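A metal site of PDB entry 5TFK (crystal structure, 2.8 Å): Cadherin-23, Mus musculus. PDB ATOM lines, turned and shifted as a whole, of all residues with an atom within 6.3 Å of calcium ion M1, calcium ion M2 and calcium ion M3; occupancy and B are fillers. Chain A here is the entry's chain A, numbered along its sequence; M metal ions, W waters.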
ATOM      1  N   GLU A  23       1.085 -15.165  28.882  1.00  0.00           N
ATOM      2  CA  GLU A  23       0.986 -13.699  29.054  1.00  0.00           C
ATOM      3  C   GLU A  23       0.748 -13.221  30.503  1.00  0.00           C
ATOM      4  O   GLU A  23       0.215 -13.962  31.337  1.00  0.00           O
ATOM      5  CB  GLU A  23      -0.100 -13.081  28.129  1.00  0.00           C
ATOM      6  CG  GLU A  23      -1.549 -13.433  28.498  1.00  0.00           C
ATOM      7  CD  GLU A  23      -2.620 -12.540  27.849  1.00  0.00           C
ATOM      8  OE1 GLU A  23      -3.821 -12.908  27.904  1.00  0.00           O
ATOM      9  OE2 GLU A  23      -2.278 -11.473  27.293  1.00  0.00           O
ATOM     10  N   ASN A  24       1.152 -11.973  30.796  1.00  0.00           N
ATOM     11  CA  ASN A  24       1.109 -11.430  32.168  1.00  0.00           C
ATOM     12  C   ASN A  24       1.912 -12.269  33.158  1.00  0.00           C
ATOM     13  O   ASN A  24       1.584 -12.302  34.349  1.00  0.00           O
ATOM     14  CB  ASN A  24      -0.333 -11.303  32.711  1.00  0.00           C
ATOM     15  CG  ASN A  24      -1.256 -10.540  31.785  1.00  0.00           C
ATOM     16  OD1 ASN A  24      -0.931  -9.422  31.363  1.00  0.00           O
ATOM     17  ND2 ASN A  24      -2.397 -11.134  31.468  1.00  0.00           N
ATOM     18  N   ILE A  80       3.818  -8.392  29.235  1.00  0.00           N
ATOM     19  CA  ILE A  80       3.531  -9.051  27.968  1.00  0.00           C
ATOM     20  C   ILE A  80       2.033  -9.311  27.832  1.00  0.00           C
ATOM     21  O   ILE A  80       1.442  -9.940  28.752  1.00  0.00           O
ATOM     22  CB  ILE A  80       4.272 -10.384  27.851  1.00  0.00           C
ATOM     23  CG1 ILE A  80       5.778 -10.158  28.028  1.00  0.00           C
ATOM     24  CG2 ILE A  80       3.968 -11.048  26.503  1.00  0.00           C
ATOM     25  CD1 ILE A  80       6.610 -11.413  28.020  1.00  0.00           C
ATOM     26  N   ASP A  81       1.463  -8.831  26.723  1.00  0.00           N
ATOM     27  CA  ASP A  81       0.014  -8.805  26.517  1.00  0.00           C
ATOM     28  C   ASP A  81      -0.341  -9.442  25.191  1.00  0.00           C
ATOM     29  O   ASP A  81       0.121  -8.959  24.183  1.00  0.00           O
ATOM     30  CB  ASP A  81      -0.433  -7.347  26.485  1.00  0.00           C
ATOM     31  CG  ASP A  81      -1.842  -7.184  25.994  1.00  0.00           C
ATOM     32  OD1 ASP A  81      -2.647  -8.126  26.157  1.00  0.00           O
ATOM     33  OD2 ASP A  81      -2.161  -6.100  25.488  1.00  0.00           O
ATOM     34  N   ARG A  82      -1.137 -10.518  25.193  1.00  0.00           N
ATOM     35  CA  ARG A  82      -1.331 -11.309  23.988  1.00  0.00           C
ATOM     36  C   ARG A  82      -2.227 -10.564  23.004  1.00  0.00           C
ATOM     37  O   ARG A  82      -2.194 -10.803  21.787  1.00  0.00           O
ATOM     38  CB  ARG A  82      -1.937 -12.659  24.379  1.00  0.00           C
ATOM     39  CG  ARG A  82      -1.806 -13.726  23.307  1.00  0.00           C
ATOM     40  CD  ARG A  82      -2.771 -14.883  23.535  1.00  0.00           C
ATOM     41  NE  ARG A  82      -4.138 -14.386  23.624  1.00  0.00           N
ATOM     42  CZ  ARG A  82      -4.855 -13.950  22.591  1.00  0.00           C
ATOM     43  NH1 ARG A  82      -4.370 -13.955  21.345  1.00  0.00           N
ATOM     44  NH2 ARG A  82      -6.090 -13.503  22.802  1.00  0.00           N
ATOM     45  N   GLU A  83      -3.031  -9.649  23.542  1.00  0.00           N
ATOM     46  CA  GLU A  83      -3.979  -8.838  22.786  1.00  0.00           C
ATOM     47  C   GLU A  83      -3.247  -7.741  22.019  1.00  0.00           C
ATOM     48  O   GLU A  83      -3.867  -7.042  21.226  1.00  0.00           O
ATOM     49  CB  GLU A  83      -4.997  -8.179  23.728  1.00  0.00           C
ATOM     50  CG  GLU A  83      -6.049  -9.100  24.345  1.00  0.00           C
ATOM     51  CD  GLU A  83      -5.469 -10.248  25.164  1.00  0.00           C
ATOM     52  OE1 GLU A  83      -5.048 -10.051  26.322  1.00  0.00           O
ATOM     53  OE2 GLU A  83      -5.451 -11.367  24.620  1.00  0.00           O
ATOM     54  N   ALA A  84      -1.950  -7.552  22.291  1.00  0.00           N
ATOM     55  CA  ALA A  84      -1.144  -6.558  21.573  1.00  0.00           C
ATOM     56  C   ALA A  84      -0.259  -7.181  20.480  1.00  0.00           C
ATOM     57  O   ALA A  84       0.490  -6.463  19.819  1.00  0.00           O
ATOM     58  CB  ALA A  84      -0.301  -5.780  22.566  1.00  0.00           C
ATOM     59  N   LEU A 113       0.799 -17.572  25.228  1.00  0.00           N
ATOM     60  CA  LEU A 113      -0.424 -18.274  25.489  1.00  0.00           C
ATOM     61  C   LEU A 113      -1.423 -17.307  26.091  1.00  0.00           C
ATOM     62  O   LEU A 113      -1.057 -16.228  26.579  1.00  0.00           O
ATOM     63  CB  LEU A 113      -0.185 -19.476  26.398  1.00  0.00           C
ATOM     64  CG  LEU A 113       0.580 -20.629  25.735  1.00  0.00           C
ATOM     65  CD1 LEU A 113       1.468 -21.302  26.757  1.00  0.00           C
ATOM     66  CD2 LEU A 113      -0.359 -21.643  25.065  1.00  0.00           C
ATOM     67  N   ASP A 114      -2.688 -17.710  26.102  1.00  0.00           N
ATOM     68  CA  ASP A 114      -3.807 -16.824  26.429  1.00  0.00           C
ATOM     69  C   ASP A 114      -4.217 -16.960  27.877  1.00  0.00           C
ATOM     70  O   ASP A 114      -4.437 -18.064  28.368  1.00  0.00           O
ATOM     71  CB  ASP A 114      -5.009 -17.124  25.552  1.00  0.00           C
ATOM     72  CG  ASP A 114      -6.100 -16.061  25.662  1.00  0.00           C
ATOM     73  OD1 ASP A 114      -5.755 -14.859  25.769  1.00  0.00           O
ATOM     74  OD2 ASP A 114      -7.289 -16.432  25.648  1.00  0.00           O
ATOM     75  N   ASP A 115      -4.292 -15.812  28.542  1.00  0.00           N
ATOM     76  CA  ASP A 115      -4.809 -15.676  29.892  1.00  0.00           C
ATOM     77  C   ASP A 115      -6.173 -14.979  29.811  1.00  0.00           C
ATOM     78  O   ASP A 115      -6.334 -14.033  29.048  1.00  0.00           O
ATOM     79  CB  ASP A 115      -3.830 -14.825  30.706  1.00  0.00           C
ATOM     80  CG  ASP A 115      -4.270 -14.605  32.137  1.00  0.00           C
ATOM     81  OD1 ASP A 115      -4.989 -15.459  32.706  1.00  0.00           O
ATOM     82  OD2 ASP A 115      -3.857 -13.560  32.684  1.00  0.00           O
ATOM     83  N   ASN A 116      -7.136 -15.439  30.580  1.00  0.00           N
ATOM     84  CA  ASN A 116      -8.470 -14.905  30.503  1.00  0.00           C
ATOM     85  C   ASN A 116      -8.498 -13.561  31.215  1.00  0.00           C
ATOM     86  O   ASN A 116      -8.980 -13.481  32.339  1.00  0.00           O
ATOM     87  CB  ASN A 116      -9.468 -15.876  31.128  1.00  0.00           C
ATOM     88  CG  ASN A 116     -10.896 -15.521  30.806  1.00  0.00           C
ATOM     89  OD1 ASN A 116     -11.180 -14.910  29.779  1.00  0.00           O
ATOM     90  ND2 ASN A 116     -11.819 -15.892  31.700  1.00  0.00           N
ATOM     91  N   ASP A 117      -7.976 -12.538  30.544  1.00  0.00           N
ATOM     92  CA  ASP A 117      -7.728 -11.206  31.163  1.00  0.00           C
ATOM     93  C   ASP A 117      -8.611 -10.071  30.663  1.00  0.00           C
ATOM     94  O   ASP A 117      -8.396  -8.912  31.015  1.00  0.00           O
ATOM     95  CB  ASP A 117      -6.250 -10.785  31.072  1.00  0.00           C
ATOM     96  CG  ASP A 117      -5.736 -10.584  29.645  1.00  0.00           C
ATOM     97  OD1 ASP A 117      -6.255 -11.178  28.682  1.00  0.00           O
ATOM     98  OD2 ASP A 117      -4.721  -9.862  29.496  1.00  0.00           O
ATOM     99  N   ASN A 118      -9.606 -10.418  29.848  1.00  0.00           N
ATOM    100  CA  ASN A 118     -10.523  -9.446  29.254  1.00  0.00           C
ATOM    101  C   ASN A 118     -11.973  -9.856  29.552  1.00  0.00           C
ATOM    102  O   ASN A 118     -12.352 -11.008  29.332  1.00  0.00           O
ATOM    103  CB  ASN A 118     -10.323  -9.379  27.735  1.00  0.00           C
ATOM    104  CG  ASN A 118      -9.128  -8.532  27.331  1.00  0.00           C
ATOM    105  OD1 ASN A 118      -9.291  -7.410  26.903  1.00  0.00           O
ATOM    106  ND2 ASN A 118      -7.925  -9.105  27.410  1.00  0.00           N
ATOM    107  N   TRP A 119     -12.767  -8.882  29.992  1.00  0.00           N
ATOM    108  CA  TRP A 119     -14.149  -9.054  30.372  1.00  0.00           C
ATOM    109  C   TRP A 119     -15.034  -8.980  29.119  1.00  0.00           C
ATOM    110  O   TRP A 119     -14.917  -8.064  28.280  1.00  0.00           O
ATOM    111  CB  TRP A 119     -14.625  -7.950  31.311  1.00  0.00           C
ATOM    112  CG  TRP A 119     -14.211  -8.095  32.727  1.00  0.00           C
ATOM    113  CD1 TRP A 119     -14.966  -8.557  33.754  1.00  0.00           C
ATOM    114  CD2 TRP A 119     -12.953  -7.720  33.287  1.00  0.00           C
ATOM    115  NE1 TRP A 119     -14.254  -8.504  34.920  1.00  0.00           N
ATOM    116  CE2 TRP A 119     -13.013  -8.000  34.656  1.00  0.00           C
ATOM    117  CE3 TRP A 119     -11.784  -7.183  32.754  1.00  0.00           C
ATOM    118  CZ2 TRP A 119     -11.939  -7.749  35.515  1.00  0.00           C
ATOM    119  CZ3 TRP A 119     -10.717  -6.921  33.601  1.00  0.00           C
ATOM    120  CH2 TRP A 119     -10.806  -7.210  34.971  1.00  0.00           C
ATOM    121  N   PRO A 120     -15.966  -9.917  28.996  1.00  0.00           N
ATOM    122  CA  PRO A 120     -17.107  -9.690  28.074  1.00  0.00           C
ATOM    123  C   PRO A 120     -17.692  -8.295  28.317  1.00  0.00           C
ATOM    124  O   PRO A 120     -17.998  -7.940  29.462  1.00  0.00           O
ATOM    125  CB  PRO A 120     -18.102 -10.786  28.470  1.00  0.00           C
ATOM    126  CG  PRO A 120     -17.254 -11.876  29.024  1.00  0.00           C
ATOM    127  CD  PRO A 120     -16.103 -11.197  29.730  1.00  0.00           C
ATOM    128  N   ASP A 148     -15.345  -9.896  23.659  1.00  0.00           N
ATOM    129  CA  ASP A 148     -14.223 -10.272  24.533  1.00  0.00           C
ATOM    130  C   ASP A 148     -12.929 -10.392  23.710  1.00  0.00           C
ATOM    131  O   ASP A 148     -12.910 -11.126  22.711  1.00  0.00           O
ATOM    132  CB  ASP A 148     -14.597 -11.623  25.184  1.00  0.00           C
ATOM    133  CG  ASP A 148     -13.666 -12.034  26.333  1.00  0.00           C
ATOM    134  OD1 ASP A 148     -12.427 -11.842  26.240  1.00  0.00           O
ATOM    135  OD2 ASP A 148     -14.161 -12.622  27.318  1.00  0.00           O
ATOM    136  N   GLU A 149     -11.914  -9.615  24.082  1.00  0.00           N
ATOM    137  CA  GLU A 149     -10.701  -9.532  23.304  1.00  0.00           C
ATOM    138  C   GLU A 149      -9.879 -10.800  23.436  1.00  0.00           C
ATOM    139  O   GLU A 149      -8.983 -10.992  22.652  1.00  0.00           O
ATOM    140  CB  GLU A 149      -9.837  -8.333  23.682  1.00  0.00           C
ATOM    141  CG  GLU A 149     -10.531  -6.984  23.580  1.00  0.00           C
ATOM    142  CD  GLU A 149     -11.319  -6.804  22.296  1.00  0.00           C
ATOM    143  OE1 GLU A 149     -10.724  -6.389  21.273  1.00  0.00           O
ATOM    144  OE2 GLU A 149     -12.546  -7.052  22.314  1.00  0.00           O
ATOM    145  N   ASP A 150     -10.188 -11.670  24.384  1.00  0.00           N
ATOM    146  CA  ASP A 150      -9.502 -12.955  24.481  1.00  0.00           C
ATOM    147  C   ASP A 150      -9.950 -13.909  23.368  1.00  0.00           C
ATOM    148  O   ASP A 150     -10.751 -13.551  22.487  1.00  0.00           O
ATOM    149  CB  ASP A 150      -9.709 -13.568  25.867  1.00  0.00           C
ATOM    150  CG  ASP A 150      -9.254 -12.641  26.984  1.00  0.00           C
ATOM    151  OD1 ASP A 150      -8.230 -11.948  26.785  1.00  0.00           O
ATOM    152  OD2 ASP A 150      -9.918 -12.610  28.054  1.00  0.00           O
ATOM    153  N   SER A 151      -9.373 -15.112  23.358  1.00  0.00           N
ATOM    154  CA  SER A 151      -9.597 -16.056  22.263  1.00  0.00           C
ATOM    155  C   SER A 151      -9.392 -17.493  22.704  1.00  0.00           C
ATOM    156  O   SER A 151      -8.672 -17.772  23.657  1.00  0.00           O
ATOM    157  CB  SER A 151      -8.708 -15.733  21.054  1.00  0.00           C
ATOM    158  OG  SER A 151      -7.338 -15.698  21.423  1.00  0.00           O
ATOM    159  N   LEU A 153     -11.675 -20.477  24.318  1.00  0.00           N
ATOM    160  CA  LEU A 153     -12.791 -20.506  25.266  1.00  0.00           C
ATOM    161  C   LEU A 153     -12.844 -19.219  26.114  1.00  0.00           C
ATOM    162  O   LEU A 153     -13.907 -18.860  26.621  1.00  0.00           O
ATOM    163  CB  LEU A 153     -12.687 -21.733  26.175  1.00  0.00           C
ATOM    164  CG  LEU A 153     -12.737 -23.120  25.514  1.00  0.00           C
ATOM    165  CD1 LEU A 153     -12.383 -24.235  26.501  1.00  0.00           C
ATOM    166  CD2 LEU A 153     -14.098 -23.371  24.865  1.00  0.00           C
ATOM    167  N   ASN A 154     -11.711 -18.526  26.217  1.00  0.00           N
ATOM    168  CA  ASN A 154     -11.636 -17.243  26.922  1.00  0.00           C
ATOM    169  C   ASN A 154     -12.402 -16.108  26.249  1.00  0.00           C
ATOM    170  O   ASN A 154     -12.666 -15.097  26.879  1.00  0.00           O
ATOM    171  CB  ASN A 154     -10.175 -16.815  27.055  1.00  0.00           C
ATOM    172  CG  ASN A 154      -9.351 -17.785  27.879  1.00  0.00           C
ATOM    173  OD1 ASN A 154      -9.880 -18.688  28.561  1.00  0.00           O
ATOM    174  ND2 ASN A 154      -8.039 -17.600  27.828  1.00  0.00           N
ATOM    175  N   GLY A 155     -12.682 -16.253  24.949  1.00  0.00           N
ATOM    176  CA  GLY A 155     -13.439 -15.250  24.192  1.00  0.00           C
ATOM    177  C   GLY A 155     -14.850 -15.638  23.765  1.00  0.00           C
ATOM    178  O   GLY A 155     -15.590 -14.807  23.261  1.00  0.00           O
ATOM    179  N   LEU A 157     -18.706 -16.755  24.177  1.00  0.00           N
ATOM    180  CA  LEU A 157     -19.646 -16.052  25.068  1.00  0.00           C
ATOM    181  C   LEU A 157     -21.006 -16.726  25.104  1.00  0.00           C
ATOM    182  O   LEU A 157     -21.594 -16.973  24.063  1.00  0.00           O
ATOM    183  CB  LEU A 157     -19.849 -14.605  24.601  1.00  0.00           C
ATOM    184  CG  LEU A 157     -18.638 -13.676  24.563  1.00  0.00           C
ATOM    185  CD1 LEU A 157     -19.069 -12.236  24.332  1.00  0.00           C
ATOM    186  CD2 LEU A 157     -17.842 -13.807  25.852  1.00  0.00           C
ATOM    187  N   ASP A 201     -17.892 -15.426  29.450  1.00  0.00           N
ATOM    188  CA  ASP A 201     -16.926 -16.321  28.805  1.00  0.00           C
ATOM    189  C   ASP A 201     -16.750 -17.704  29.449  1.00  0.00           C
ATOM    190  O   ASP A 201     -17.262 -18.006  30.542  1.00  0.00           O
ATOM    191  CB  ASP A 201     -15.559 -15.622  28.572  1.00  0.00           C
ATOM    192  CG  ASP A 201     -14.790 -15.321  29.853  1.00  0.00           C
ATOM    193  OD1 ASP A 201     -14.915 -16.031  30.876  1.00  0.00           O
ATOM    194  OD2 ASP A 201     -13.988 -14.366  29.840  1.00  0.00           O
ATOM    195  N   GLY A 203     -13.533 -19.176  30.059  1.00  0.00           N
ATOM    196  CA  GLY A 203     -12.220 -19.356  30.687  1.00  0.00           C
ATOM    197  C   GLY A 203     -12.393 -20.035  32.026  1.00  0.00           C
ATOM    198  O   GLY A 203     -13.471 -19.953  32.631  1.00  0.00           O
ATOM    199  N   LEU A 207     -15.114 -14.996  33.411  1.00  0.00           N
ATOM    200  CA  LEU A 207     -15.434 -13.566  33.540  1.00  0.00           C
ATOM    201  C   LEU A 207     -16.754 -13.170  32.839  1.00  0.00           C
ATOM    202  O   LEU A 207     -17.135 -13.736  31.809  1.00  0.00           O
ATOM    203  CB  LEU A 207     -14.306 -12.688  32.974  1.00  0.00           C
ATOM    204  CG  LEU A 207     -12.989 -12.561  33.753  1.00  0.00           C
ATOM    205  CD1 LEU A 207     -11.935 -11.862  32.914  1.00  0.00           C
ATOM    206  CD2 LEU A 207     -13.186 -11.807  35.050  1.00  0.00           C
HETATM  207 CA    CA M   1     -12.294 -13.298  28.647  1.00  0.00          CA
HETATM  208 CA    CA M   2      -5.933 -12.804  27.060  1.00  0.00          CA
HETATM  209 CA    CA M   3      -3.427  -9.273  27.990  1.00  0.00          CA
HETATM  210  O   HOH W   1      -5.072  -7.650  27.809  1.00  0.00           O
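The side-chain carboxylate of Asp 115 sits at hydrogen-bond distance from the side-chain amide nitrogen of Asn 24, 3.1 Å away.
The side-chain amide nitrogen of Asn 118 sits close to the side-chain carboxylate of Asp 117 (3.0 Å).
The side-chain carboxylate (OD2) of Asp 114 is in hydrogen-bond range of the backbone NH (N) of Ser 151, at 3.4 Å.
The side-chain carboxylate of Asp 117 lies close to the side-chain amide nitrogen of Asn 24.
OD1 of Asp 201 lies within hydrogen-bond range of N of Leu 207 (2.7 Å).
NH2 of Arg 82 lies within hydrogen-bond range of OG of Ser 151 (2.9 Å).
The guanidinium group of Arg 82 sits close to the side-chain carboxylate of Glu 83, 2.9 Å away.
The backbone NH (N) of Glu 23 is in hydrogen-bond range of the backbone carbonyl oxygen (O) of Leu 113.
Six residues have an atom within 4 Å of calcium ion M2: Glu 23, Glu 83, Asp 114, Asp 115, Asp 117 and Asp 150.
Arg 82 touches calcium ion M3 (N to CA, 3.8 Å).
Of the 26 residues printed, 5 come within 4 Å of calcium ion M3.
The nearest printed residue that does not touch calcium ion M3 is Asn 24 (4.1 Å).
Calcium ion M1 is bound by OD1 of Asn 116, OD2 of Asp 201, OD2 of Asp 148, O of Asn 118, OD2 of Asp 150, O of Asn 154 and OD1 of Asp 148.
Calcium ion M1 has seven donor atoms within binding distance.
Calcium ion M2 is bound by OE1 of Glu 23 (2.3 Å), OD1 of Asp 117 (2.3 Å), O of Asp 115 (2.4 Å), OD1 of Asp 114 (2.4 Å), OD1 of Asp 150 (2.5 Å) and OE2 of Glu 83 (2.9 Å).
Slightly farther from calcium ion M2 lies OE1 of Glu 83 (3.0 Å).
Calcium ion M3 is bound by OD2 of Asp 117 (2.1 Å), OD1 of Asp 81 (2.3 Å), water W1 (2.3 Å), OE1 of Glu 83 (2.5 Å) and OE2 of Glu 23 (2.6 Å).
Calcium ion M3 has five donor atoms within binding distance.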
